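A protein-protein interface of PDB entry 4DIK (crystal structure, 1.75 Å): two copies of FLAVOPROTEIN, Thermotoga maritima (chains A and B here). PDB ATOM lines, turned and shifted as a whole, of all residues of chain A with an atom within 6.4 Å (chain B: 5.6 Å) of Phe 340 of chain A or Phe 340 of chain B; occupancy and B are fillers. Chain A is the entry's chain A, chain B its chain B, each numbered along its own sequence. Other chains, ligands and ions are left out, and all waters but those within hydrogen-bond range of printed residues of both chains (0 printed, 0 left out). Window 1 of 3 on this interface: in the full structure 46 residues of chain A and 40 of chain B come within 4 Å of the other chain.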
ATOM      1  N   VAL A  43       4.610  -4.560 -15.633  1.00  0.00           N
ATOM      2  CA  VAL A  43       6.075  -4.578 -15.812  1.00  0.00           C
ATOM      3  C   VAL A  43       6.538  -5.085 -17.177  1.00  0.00           C
ATOM      4  O   VAL A  43       7.432  -4.509 -17.785  1.00  0.00           O
ATOM      5  CB  VAL A  43       6.783  -5.392 -14.688  1.00  0.00           C
ATOM      6  CG1 VAL A  43       6.130  -6.711 -14.472  1.00  0.00           C
ATOM      7  CG2 VAL A  43       8.299  -5.538 -14.963  1.00  0.00           C
ATOM      8  N   TRP A  44       5.933  -6.164 -17.673  1.00  0.00           N
ATOM      9  CA  TRP A  44       6.500  -6.797 -18.871  1.00  0.00           C
ATOM     10  C   TRP A  44       5.986  -6.183 -20.156  1.00  0.00           C
ATOM     11  O   TRP A  44       4.785  -6.210 -20.415  1.00  0.00           O
ATOM     12  CB  TRP A  44       6.273  -8.309 -18.855  1.00  0.00           C
ATOM     13  CG  TRP A  44       6.570  -8.880 -17.540  1.00  0.00           C
ATOM     14  CD1 TRP A  44       5.687  -9.490 -16.704  1.00  0.00           C
ATOM     15  CD2 TRP A  44       7.838  -8.896 -16.873  1.00  0.00           C
ATOM     16  NE1 TRP A  44       6.329  -9.897 -15.560  1.00  0.00           N
ATOM     17  CE2 TRP A  44       7.643  -9.537 -15.635  1.00  0.00           C
ATOM     18  CE3 TRP A  44       9.121  -8.442 -17.209  1.00  0.00           C
ATOM     19  CZ2 TRP A  44       8.680  -9.726 -14.721  1.00  0.00           C
ATOM     20  CZ3 TRP A  44      10.158  -8.639 -16.297  1.00  0.00           C
ATOM     21  CH2 TRP A  44       9.922  -9.271 -15.063  1.00  0.00           C
ATOM     22  N   ILE A 310      13.021  -5.287 -21.202  1.00  0.00           N
ATOM     23  CA  ILE A 310      13.479  -6.398 -20.369  1.00  0.00           C
ATOM     24  C   ILE A 310      12.754  -7.713 -20.718  1.00  0.00           C
ATOM     25  O   ILE A 310      13.355  -8.802 -20.678  1.00  0.00           O
ATOM     26  CB  ILE A 310      13.356  -6.091 -18.846  1.00  0.00           C
ATOM     27  CG1 ILE A 310      14.019  -7.186 -18.007  1.00  0.00           C
ATOM     28  CG2 ILE A 310      11.907  -5.957 -18.418  1.00  0.00           C
ATOM     29  CD1 ILE A 310      15.518  -7.300 -18.216  1.00  0.00           C
ATOM     30  N   ILE A 334      27.651  -1.479 -10.633  1.00  0.00           N
ATOM     31  CA  ILE A 334      26.546  -1.848 -11.494  1.00  0.00           C
ATOM     32  C   ILE A 334      25.630  -0.642 -11.715  1.00  0.00           C
ATOM     33  O   ILE A 334      25.095  -0.051 -10.777  1.00  0.00           O
ATOM     34  CB  ILE A 334      25.769  -3.068 -10.955  1.00  0.00           C
ATOM     35  CG1 ILE A 334      26.755  -4.152 -10.476  1.00  0.00           C
ATOM     36  CG2 ILE A 334      24.866  -3.626 -12.039  1.00  0.00           C
ATOM     37  CD1 ILE A 334      26.152  -5.250  -9.621  1.00  0.00           C
ATOM     38  N   HIS A 335      25.471  -0.276 -12.975  1.00  0.00           N
ATOM     39  CA  HIS A 335      24.615   0.843 -13.314  1.00  0.00           C
ATOM     40  C   HIS A 335      23.176   0.411 -13.490  1.00  0.00           C
ATOM     41  O   HIS A 335      22.921  -0.730 -13.882  1.00  0.00           O
ATOM     42  CB  HIS A 335      25.206   1.602 -14.496  1.00  0.00           C
ATOM     43  CG  HIS A 335      26.355   2.458 -14.091  1.00  0.00           C
ATOM     44  ND1 HIS A 335      26.193   3.743 -13.622  1.00  0.00           N
ATOM     45  CD2 HIS A 335      27.678   2.184 -13.993  1.00  0.00           C
ATOM     46  CE1 HIS A 335      27.369   4.239 -13.292  1.00  0.00           C
ATOM     47  NE2 HIS A 335      28.288   3.314 -13.508  1.00  0.00           N
ATOM     48  N   PRO A 336      22.236   1.313 -13.156  1.00  0.00           N
ATOM     49  CA  PRO A 336      20.856   0.953 -12.829  1.00  0.00           C
ATOM     50  C   PRO A 336      20.168  -0.013 -13.793  1.00  0.00           C
ATOM     51  O   PRO A 336      19.558  -0.950 -13.311  1.00  0.00           O
ATOM     52  CB  PRO A 336      20.139   2.309 -12.782  1.00  0.00           C
ATOM     53  CG  PRO A 336      21.223   3.250 -12.373  1.00  0.00           C
ATOM     54  CD  PRO A 336      22.441   2.778 -13.091  1.00  0.00           C
ATOM     55  N   LEU A 337      20.282   0.186 -15.103  1.00  0.00           N
ATOM     56  CA  LEU A 337      19.597  -0.713 -16.030  1.00  0.00           C
ATOM     57  C   LEU A 337      20.224  -2.104 -16.090  1.00  0.00           C
ATOM     58  O   LEU A 337      19.511  -3.093 -16.228  1.00  0.00           O
ATOM     59  CB  LEU A 337      19.505  -0.115 -17.416  1.00  0.00           C
ATOM     60  CG  LEU A 337      18.673   1.160 -17.343  1.00  0.00           C
ATOM     61  CD1 LEU A 337      18.898   1.869 -18.622  1.00  0.00           C
ATOM     62  CD2 LEU A 337      17.208   0.804 -17.152  1.00  0.00           C
ATOM     63  N   MET A 338      21.551  -2.155 -15.985  1.00  0.00           N
ATOM     64  CA  MET A 338      22.266  -3.423 -15.903  1.00  0.00           C
ATOM     65  C   MET A 338      21.847  -4.174 -14.645  1.00  0.00           C
ATOM     66  O   MET A 338      21.608  -5.379 -14.677  1.00  0.00           O
ATOM     67  CB  MET A 338      23.779  -3.185 -15.908  1.00  0.00           C
ATOM     68  CG  MET A 338      24.604  -4.456 -15.832  1.00  0.00           C
ATOM     69  SD  MET A 338      24.041  -5.685 -17.030  1.00  0.00           S
ATOM     70  CE  MET A 338      24.266  -4.830 -18.586  1.00  0.00           C
ATOM     71  N   ARG A 339      21.750  -3.447 -13.538  1.00  0.00           N
ATOM     72  CA  ARG A 339      21.346  -4.040 -12.256  1.00  0.00           C
ATOM     73  C   ARG A 339      19.934  -4.619 -12.346  1.00  0.00           C
ATOM     74  O   ARG A 339      19.680  -5.766 -11.920  1.00  0.00           O
ATOM     75  CB  ARG A 339      21.432  -3.017 -11.115  1.00  0.00           C
ATOM     76  CG  ARG A 339      21.082  -3.609  -9.754  1.00  0.00           C
ATOM     77  CD  ARG A 339      20.769  -2.538  -8.699  1.00  0.00           C
ATOM     78  NE  ARG A 339      19.574  -1.773  -9.042  1.00  0.00           N
ATOM     79  CZ  ARG A 339      19.542  -0.455  -9.214  1.00  0.00           C
ATOM     80  NH1 ARG A 339      20.643   0.269  -9.050  1.00  0.00           N
ATOM     81  NH2 ARG A 339      18.392   0.142  -9.528  1.00  0.00           N
ATOM     82  N   PHE A 340      19.010  -3.830 -12.899  1.00  0.00           N
ATOM     83  CA  PHE A 340      17.634  -4.276 -13.060  1.00  0.00           C
ATOM     84  C   PHE A 340      17.621  -5.555 -13.905  1.00  0.00           C
ATOM     85  O   PHE A 340      16.947  -6.537 -13.567  1.00  0.00           O
ATOM     86  CB  PHE A 340      16.758  -3.184 -13.716  1.00  0.00           C
ATOM     87  CG  PHE A 340      15.308  -3.573 -13.837  1.00  0.00           C
ATOM     88  CD1 PHE A 340      14.433  -3.320 -12.799  1.00  0.00           C
ATOM     89  CD2 PHE A 340      14.810  -4.195 -14.988  1.00  0.00           C
ATOM     90  CE1 PHE A 340      13.078  -3.699 -12.862  1.00  0.00           C
ATOM     91  CE2 PHE A 340      13.465  -4.549 -15.082  1.00  0.00           C
ATOM     92  CZ  PHE A 340      12.584  -4.322 -14.010  1.00  0.00           C
ATOM     93  N   THR A 341      18.395  -5.531 -14.988  1.00  0.00           N
ATOM     94  CA  THR A 341      18.424  -6.624 -15.961  1.00  0.00           C
ATOM     95  C   THR A 341      19.005  -7.890 -15.324  1.00  0.00           C
ATOM     96  O   THR A 341      18.410  -8.966 -15.406  1.00  0.00           O
ATOM     97  CB  THR A 341      19.215  -6.210 -17.233  1.00  0.00           C
ATOM     98  OG1 THR A 341      18.511  -5.152 -17.902  1.00  0.00           O
ATOM     99  CG2 THR A 341      19.390  -7.406 -18.190  1.00  0.00           C
ATOM    100  N   LEU A 342      20.138  -7.750 -14.638  1.00  0.00           N
ATOM    101  CA  LEU A 342      20.695  -8.871 -13.873  1.00  0.00           C
ATOM    102  C   LEU A 342      19.763  -9.448 -12.804  1.00  0.00           C
ATOM    103  O   LEU A 342      19.652 -10.661 -12.687  1.00  0.00           O
ATOM    104  CB  LEU A 342      22.025  -8.475 -13.232  1.00  0.00           C
ATOM    105  CG  LEU A 342      23.175  -8.327 -14.222  1.00  0.00           C
ATOM    106  CD1 LEU A 342      24.385  -7.640 -13.576  1.00  0.00           C
ATOM    107  CD2 LEU A 342      23.551  -9.694 -14.762  1.00  0.00           C
ATOM    108  N   LEU A 343      19.127  -8.591 -12.011  1.00  0.00           N
ATOM    109  CA  LEU A 343      18.237  -9.063 -10.973  1.00  0.00           C
ATOM    110  C   LEU A 343      17.048  -9.831 -11.571  1.00  0.00           C
ATOM    111  O   LEU A 343      16.624 -10.841 -11.023  1.00  0.00           O
ATOM    112  CB  LEU A 343      17.743  -7.911 -10.103  1.00  0.00           C
ATOM    113  CG  LEU A 343      18.797  -7.279  -9.189  1.00  0.00           C
ATOM    114  CD1 LEU A 343      18.150  -6.134  -8.443  1.00  0.00           C
ATOM    115  CD2 LEU A 343      19.303  -8.330  -8.222  1.00  0.00           C
ATOM    116  N   GLU A 344      16.519  -9.352 -12.695  1.00  0.00           N
ATOM    117  CA  GLU A 344      15.409 -10.045 -13.338  1.00  0.00           C
ATOM    118  C   GLU A 344      15.845 -11.364 -13.970  1.00  0.00           C
ATOM    119  O   GLU A 344      15.093 -12.333 -13.972  1.00  0.00           O
ATOM    120  CB  GLU A 344      14.728  -9.147 -14.381  1.00  0.00           C
ATOM    121  CG  GLU A 344      14.051  -7.929 -13.745  1.00  0.00           C
ATOM    122  CD  GLU A 344      13.197  -8.309 -12.545  1.00  0.00           C
ATOM    123  OE1 GLU A 344      12.404  -9.272 -12.641  1.00  0.00           O
ATOM    124  OE2 GLU A 344      13.313  -7.642 -11.491  1.00  0.00           O
ATOM    125  N   ILE A 345      17.051 -11.394 -14.523  1.00  0.00           N
ATOM    126  CA  ILE A 345      17.572 -12.642 -15.063  1.00  0.00           C
ATOM    127  C   ILE A 345      17.766 -13.657 -13.954  1.00  0.00           C
ATOM    128  O   ILE A 345      17.423 -14.837 -14.091  1.00  0.00           O
ATOM    129  CB  ILE A 345      18.904 -12.402 -15.797  1.00  0.00           C
ATOM    130  CG1 ILE A 345      18.638 -11.780 -17.168  1.00  0.00           C
ATOM    131  CG2 ILE A 345      19.695 -13.712 -15.945  1.00  0.00           C
ATOM    132  CD1 ILE A 345      19.899 -11.218 -17.816  1.00  0.00           C
ATOM    133  N   VAL B  43      21.042   6.149 -18.965  1.00  0.00           N
ATOM    134  CA  VAL B  43      19.992   5.827 -18.004  1.00  0.00           C
ATOM    135  C   VAL B  43      18.911   6.904 -17.834  1.00  0.00           C
ATOM    136  O   VAL B  43      17.714   6.587 -17.812  1.00  0.00           O
ATOM    137  CB  VAL B  43      20.591   5.390 -16.642  1.00  0.00           C
ATOM    138  CG1 VAL B  43      21.581   6.402 -16.132  1.00  0.00           C
ATOM    139  CG2 VAL B  43      19.485   5.068 -15.617  1.00  0.00           C
ATOM    140  N   ILE B 310      12.057   7.459 -14.500  1.00  0.00           N
ATOM    141  CA  ILE B 310      12.700   7.562 -13.194  1.00  0.00           C
ATOM    142  C   ILE B 310      13.370   8.929 -12.991  1.00  0.00           C
ATOM    143  O   ILE B 310      13.426   9.428 -11.873  1.00  0.00           O
ATOM    144  CB  ILE B 310      13.701   6.402 -12.926  1.00  0.00           C
ATOM    145  CG1 ILE B 310      14.187   6.401 -11.470  1.00  0.00           C
ATOM    146  CG2 ILE B 310      14.894   6.476 -13.865  1.00  0.00           C
ATOM    147  CD1 ILE B 310      13.060   6.286 -10.432  1.00  0.00           C
ATOM    148  N   HIS B 335       7.104  -5.431  -6.078  1.00  0.00           N
ATOM    149  CA  HIS B 335       7.021  -5.147  -7.508  1.00  0.00           C
ATOM    150  C   HIS B 335       8.325  -4.554  -8.031  1.00  0.00           C
ATOM    151  O   HIS B 335       8.801  -3.541  -7.502  1.00  0.00           O
ATOM    152  CB  HIS B 335       5.854  -4.184  -7.759  1.00  0.00           C
ATOM    153  CG  HIS B 335       5.498  -4.017  -9.203  1.00  0.00           C
ATOM    154  ND1 HIS B 335       6.116  -3.094 -10.024  1.00  0.00           N
ATOM    155  CD2 HIS B 335       4.585  -4.652  -9.977  1.00  0.00           C
ATOM    156  CE1 HIS B 335       5.599  -3.169 -11.235  1.00  0.00           C
ATOM    157  NE2 HIS B 335       4.662  -4.103 -11.234  1.00  0.00           N
ATOM    158  N   PRO B 336       8.919  -5.190  -9.067  1.00  0.00           N
ATOM    159  CA  PRO B 336      10.212  -4.810  -9.657  1.00  0.00           C
ATOM    160  C   PRO B 336      10.403  -3.327  -9.990  1.00  0.00           C
ATOM    161  O   PRO B 336      11.515  -2.817  -9.853  1.00  0.00           O
ATOM    162  CB  PRO B 336      10.264  -5.605 -10.962  1.00  0.00           C
ATOM    163  CG  PRO B 336       9.381  -6.766 -10.743  1.00  0.00           C
ATOM    164  CD  PRO B 336       8.376  -6.423  -9.669  1.00  0.00           C
ATOM    165  N   LEU B 337       9.354  -2.661 -10.461  1.00  0.00           N
ATOM    166  CA  LEU B 337       9.479  -1.261 -10.829  1.00  0.00           C
ATOM    167  C   LEU B 337       9.544  -0.374  -9.593  1.00  0.00           C
ATOM    168  O   LEU B 337      10.217   0.660  -9.599  1.00  0.00           O
ATOM    169  CB  LEU B 337       8.355  -0.827 -11.771  1.00  0.00           C
ATOM    170  CG  LEU B 337       8.642  -1.273 -13.207  1.00  0.00           C
ATOM    171  CD1 LEU B 337       7.471  -0.953 -14.145  1.00  0.00           C
ATOM    172  CD2 LEU B 337       9.927  -0.627 -13.725  1.00  0.00           C
ATOM    173  N   MET B 338       8.849  -0.775  -8.537  1.00  0.00           N
ATOM    174  CA  MET B 338       8.973  -0.063  -7.266  1.00  0.00           C
ATOM    175  C   MET B 338      10.307  -0.360  -6.591  1.00  0.00           C
ATOM    176  O   MET B 338      10.879   0.510  -5.951  1.00  0.00           O
ATOM    177  CB  MET B 338       7.797  -0.364  -6.347  1.00  0.00           C
ATOM    178  CG  MET B 338       6.488   0.282  -6.844  1.00  0.00           C
ATOM    179  SD  MET B 338       6.521   2.064  -6.746  1.00  0.00           S
ATOM    180  CE  MET B 338       6.679   2.248  -4.968  1.00  0.00           C
ATOM    181  N   ARG B 339      10.811  -1.585  -6.754  1.00  0.00           N
ATOM    182  CA  ARG B 339      12.164  -1.889  -6.282  1.00  0.00           C
ATOM    183  C   ARG B 339      13.192  -0.975  -6.935  1.00  0.00           C
ATOM    184  O   ARG B 339      14.003  -0.337  -6.249  1.00  0.00           O
ATOM    185  CB  ARG B 339      12.557  -3.349  -6.565  1.00  0.00           C
ATOM    186  CG  ARG B 339      13.929  -3.727  -5.976  1.00  0.00           C
ATOM    187  CD  ARG B 339      14.436  -5.034  -6.541  1.00  0.00           C
ATOM    188  NE  ARG B 339      14.826  -4.892  -7.948  1.00  0.00           N
ATOM    189  CZ  ARG B 339      14.369  -5.678  -8.919  1.00  0.00           C
ATOM    190  NH1 ARG B 339      13.523  -6.657  -8.631  1.00  0.00           N
ATOM    191  NH2 ARG B 339      14.763  -5.481 -10.172  1.00  0.00           N
ATOM    192  N   PHE B 340      13.156  -0.920  -8.266  1.00  0.00           N
ATOM    193  CA  PHE B 340      14.070  -0.087  -9.027  1.00  0.00           C
ATOM    194  C   PHE B 340      13.973   1.358  -8.559  1.00  0.00           C
ATOM    195  O   PHE B 340      14.991   2.031  -8.354  1.00  0.00           O
ATOM    196  CB  PHE B 340      13.744  -0.160 -10.526  1.00  0.00           C
ATOM    197  CG  PHE B 340      14.623   0.699 -11.382  1.00  0.00           C
ATOM    198  CD1 PHE B 340      15.811   0.207 -11.897  1.00  0.00           C
ATOM    199  CD2 PHE B 340      14.260   2.004 -11.685  1.00  0.00           C
ATOM    200  CE1 PHE B 340      16.630   0.991 -12.686  1.00  0.00           C
ATOM    201  CE2 PHE B 340      15.064   2.799 -12.485  1.00  0.00           C
ATOM    202  CZ  PHE B 340      16.258   2.300 -13.000  1.00  0.00           C
ATOM    203  N   THR B 341      12.741   1.825  -8.399  1.00  0.00           N
ATOM    204  CA  THR B 341      12.492   3.217  -8.029  1.00  0.00           C
ATOM    205  C   THR B 341      12.991   3.534  -6.612  1.00  0.00           C
ATOM    206  O   THR B 341      13.650   4.561  -6.396  1.00  0.00           O
ATOM    207  CB  THR B 341      10.992   3.576  -8.205  1.00  0.00           C
ATOM    208  OG1 THR B 341      10.649   3.497  -9.595  1.00  0.00           O
ATOM    209  CG2 THR B 341      10.732   4.994  -7.744  1.00  0.00           C
ATOM    210  N   LEU B 342      12.698   2.658  -5.663  1.00  0.00           N
ATOM    211  CA  LEU B 342      13.209   2.820  -4.299  1.00  0.00           C
ATOM    212  C   LEU B 342      14.731   2.860  -4.273  1.00  0.00           C
ATOM    213  O   LEU B 342      15.329   3.753  -3.665  1.00  0.00           O
ATOM    214  CB  LEU B 342      12.674   1.716  -3.393  1.00  0.00           C
ATOM    215  CG  LEU B 342      11.195   1.876  -3.006  1.00  0.00           C
ATOM    216  CD1 LEU B 342      10.657   0.614  -2.353  1.00  0.00           C
ATOM    217  CD2 LEU B 342      11.018   3.099  -2.119  1.00  0.00           C
ATOM    218  N   LEU B 343      15.361   1.922  -4.966  1.00  0.00           N
ATOM    219  CA  LEU B 343      16.821   1.883  -4.989  1.00  0.00           C
ATOM    220  C   LEU B 343      17.453   3.161  -5.542  1.00  0.00           C
ATOM    221  O   LEU B 343      18.488   3.621  -5.042  1.00  0.00           O
ATOM    222  CB  LEU B 343      17.313   0.664  -5.757  1.00  0.00           C
ATOM    223  CG  LEU B 343      17.034  -0.677  -5.071  1.00  0.00           C
ATOM    224  CD1 LEU B 343      17.474  -1.833  -5.990  1.00  0.00           C
ATOM    225  CD2 LEU B 343      17.739  -0.766  -3.713  1.00  0.00           C
ATOM    226  N   GLU B 344      16.830   3.751  -6.559  1.00  0.00           N
ATOM    227  CA  GLU B 344      17.348   4.986  -7.125  1.00  0.00           C
ATOM    228  C   GLU B 344      17.120   6.215  -6.230  1.00  0.00           C
ATOM    229  O   GLU B 344      17.993   7.079  -6.101  1.00  0.00           O
ATOM    230  CB  GLU B 344      16.779   5.200  -8.534  1.00  0.00           C
ATOM    231  CG  GLU B 344      17.226   4.118  -9.517  1.00  0.00           C
ATOM    232  CD  GLU B 344      18.743   3.987  -9.569  1.00  0.00           C
ATOM    233  OE1 GLU B 344      19.431   5.028  -9.628  1.00  0.00           O
ATOM    234  OE2 GLU B 344      19.245   2.838  -9.550  1.00  0.00           O
ATOM    235  N   ILE B 345      15.947   6.286  -5.617  1.00  0.00           N
ATOM    236  CA  ILE B 345      15.666   7.348  -4.660  1.00  0.00           C
ATOM    237  C   ILE B 345      16.649   7.288  -3.480  1.00  0.00           C
ATOM    238  O   ILE B 345      17.187   8.310  -3.051  1.00  0.00           O
ATOM    239  CB  ILE B 345      14.220   7.250  -4.140  1.00  0.00           C
ATOM    240  CG1 ILE B 345      13.237   7.638  -5.253  1.00  0.00           C
ATOM    241  CG2 ILE B 345      14.025   8.185  -2.936  1.00  0.00           C
ATOM    242  CD1 ILE B 345      11.769   7.308  -4.913  1.00  0.00           C
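The side-chain carboxylate (OE2) of Glu 344 of chain B is in salt-bridge range of the guanidinium group (NH2) of Arg 339 of chain A.
The side-chain carboxylate (OE2) of Glu 344 of chain A is in salt-bridge range of the guanidinium group (NH2) of Arg 339 of chain B (2.9 Å).
Pro 336 of chain A touches Phe 340 of chain B (O to CE1, 3.6 Å).
Pro 336 of chain A touches Glu 344 of chain B (CB to OE2, 3.4 Å).
CD1 of Phe 340 of chain B touches NH2 of Arg 339 of chain A (3.5 Å).
NE of Arg 339 of chain A touches CD1 of Leu 343 of chain B, at 3.7 Å.
CE1 of Phe 340 of chain A touches O of Pro 336 of chain B, 3.5 Å away.
Arg 339 of chain B touches Phe 340 of chain A.
Phe 340 of chain A touches Phe 340 of chain B.
NE of Arg 339 of chain B touches CD1 of Leu 343 of chain A, 3.6 Å away.
OE2 of Glu 344 of chain A touches CB of Pro 336 of chain B, at 3.7 Å.
Phe 340 of chain A touches three residues of chain B.
Phe 340 of chain B touches just these residues of chain A: Pro 336, Arg 339 and Phe 340.
Printed residues of chain B within 4 Å of Pro 336 of chain A: Phe 340 and Glu 344.
Of the printed residues of chain A, Arg 339 of chain B touches Phe 340, Leu 343 and Glu 344.
Of the printed residues of chain A, Glu 344 of chain B touches Pro 336 (3.4 Å) and Arg 339 (2.8 Å).
Leu 342 of chain A touches none of the printed residues of chain B.
The nearest residue of chain B that does not touch Phe 340 of chain A is Leu 337 of chain B (4.5 Å).
The nearest residue of chain A that does not touch Phe 340 of chain B is Leu 337 of chain A (4.5 Å).
Of the 15 printed residues of chain A, 5 touch a printed residue of chain B.
Hydrophobic or aromatic side chains of chain A within 4 Å of the printed part of chain B: Pro 336, Phe 340 and Leu 343.
Of the 13 printed residues of chain B, 5 touch a printed residue of chain A.
Among the printed residues, Asp or Glu carboxylates within 4 Å of a Lys or Arg side-chain nitrogen of the other chain: Arg 339 of chain A with Glu 344 of chain B and Glu 344 of chain A with Arg 339 of chain B.
Pro 336 of chain A touches Phe 340 of chain B, and with the chains exchanged Phe 340 of chain A touches Pro 336 of chain B.
Pro 336 of chain A touches Glu 344 of chain B, and with the chains exchanged Glu 344 of chain A touches Pro 336 of chain B.
Arg 339 of chain A touches Phe 340 of chain B, and with the chains exchanged Phe 340 of chain A touches Arg 339 of chain B.
Arg 339 of chain A touches Glu 344 of chain B, and with the chains exchanged Glu 344 of chain A touches Arg 339 of chain B.
Positions printed for both chains: 43, 310, 335, 336, 337, 338, 339, 340, 341, 342, 343, 344 and 345.
Of the 11 pairs that touch across the chains among the printed residues, 11 have their exchanged pair printed and touching as well.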
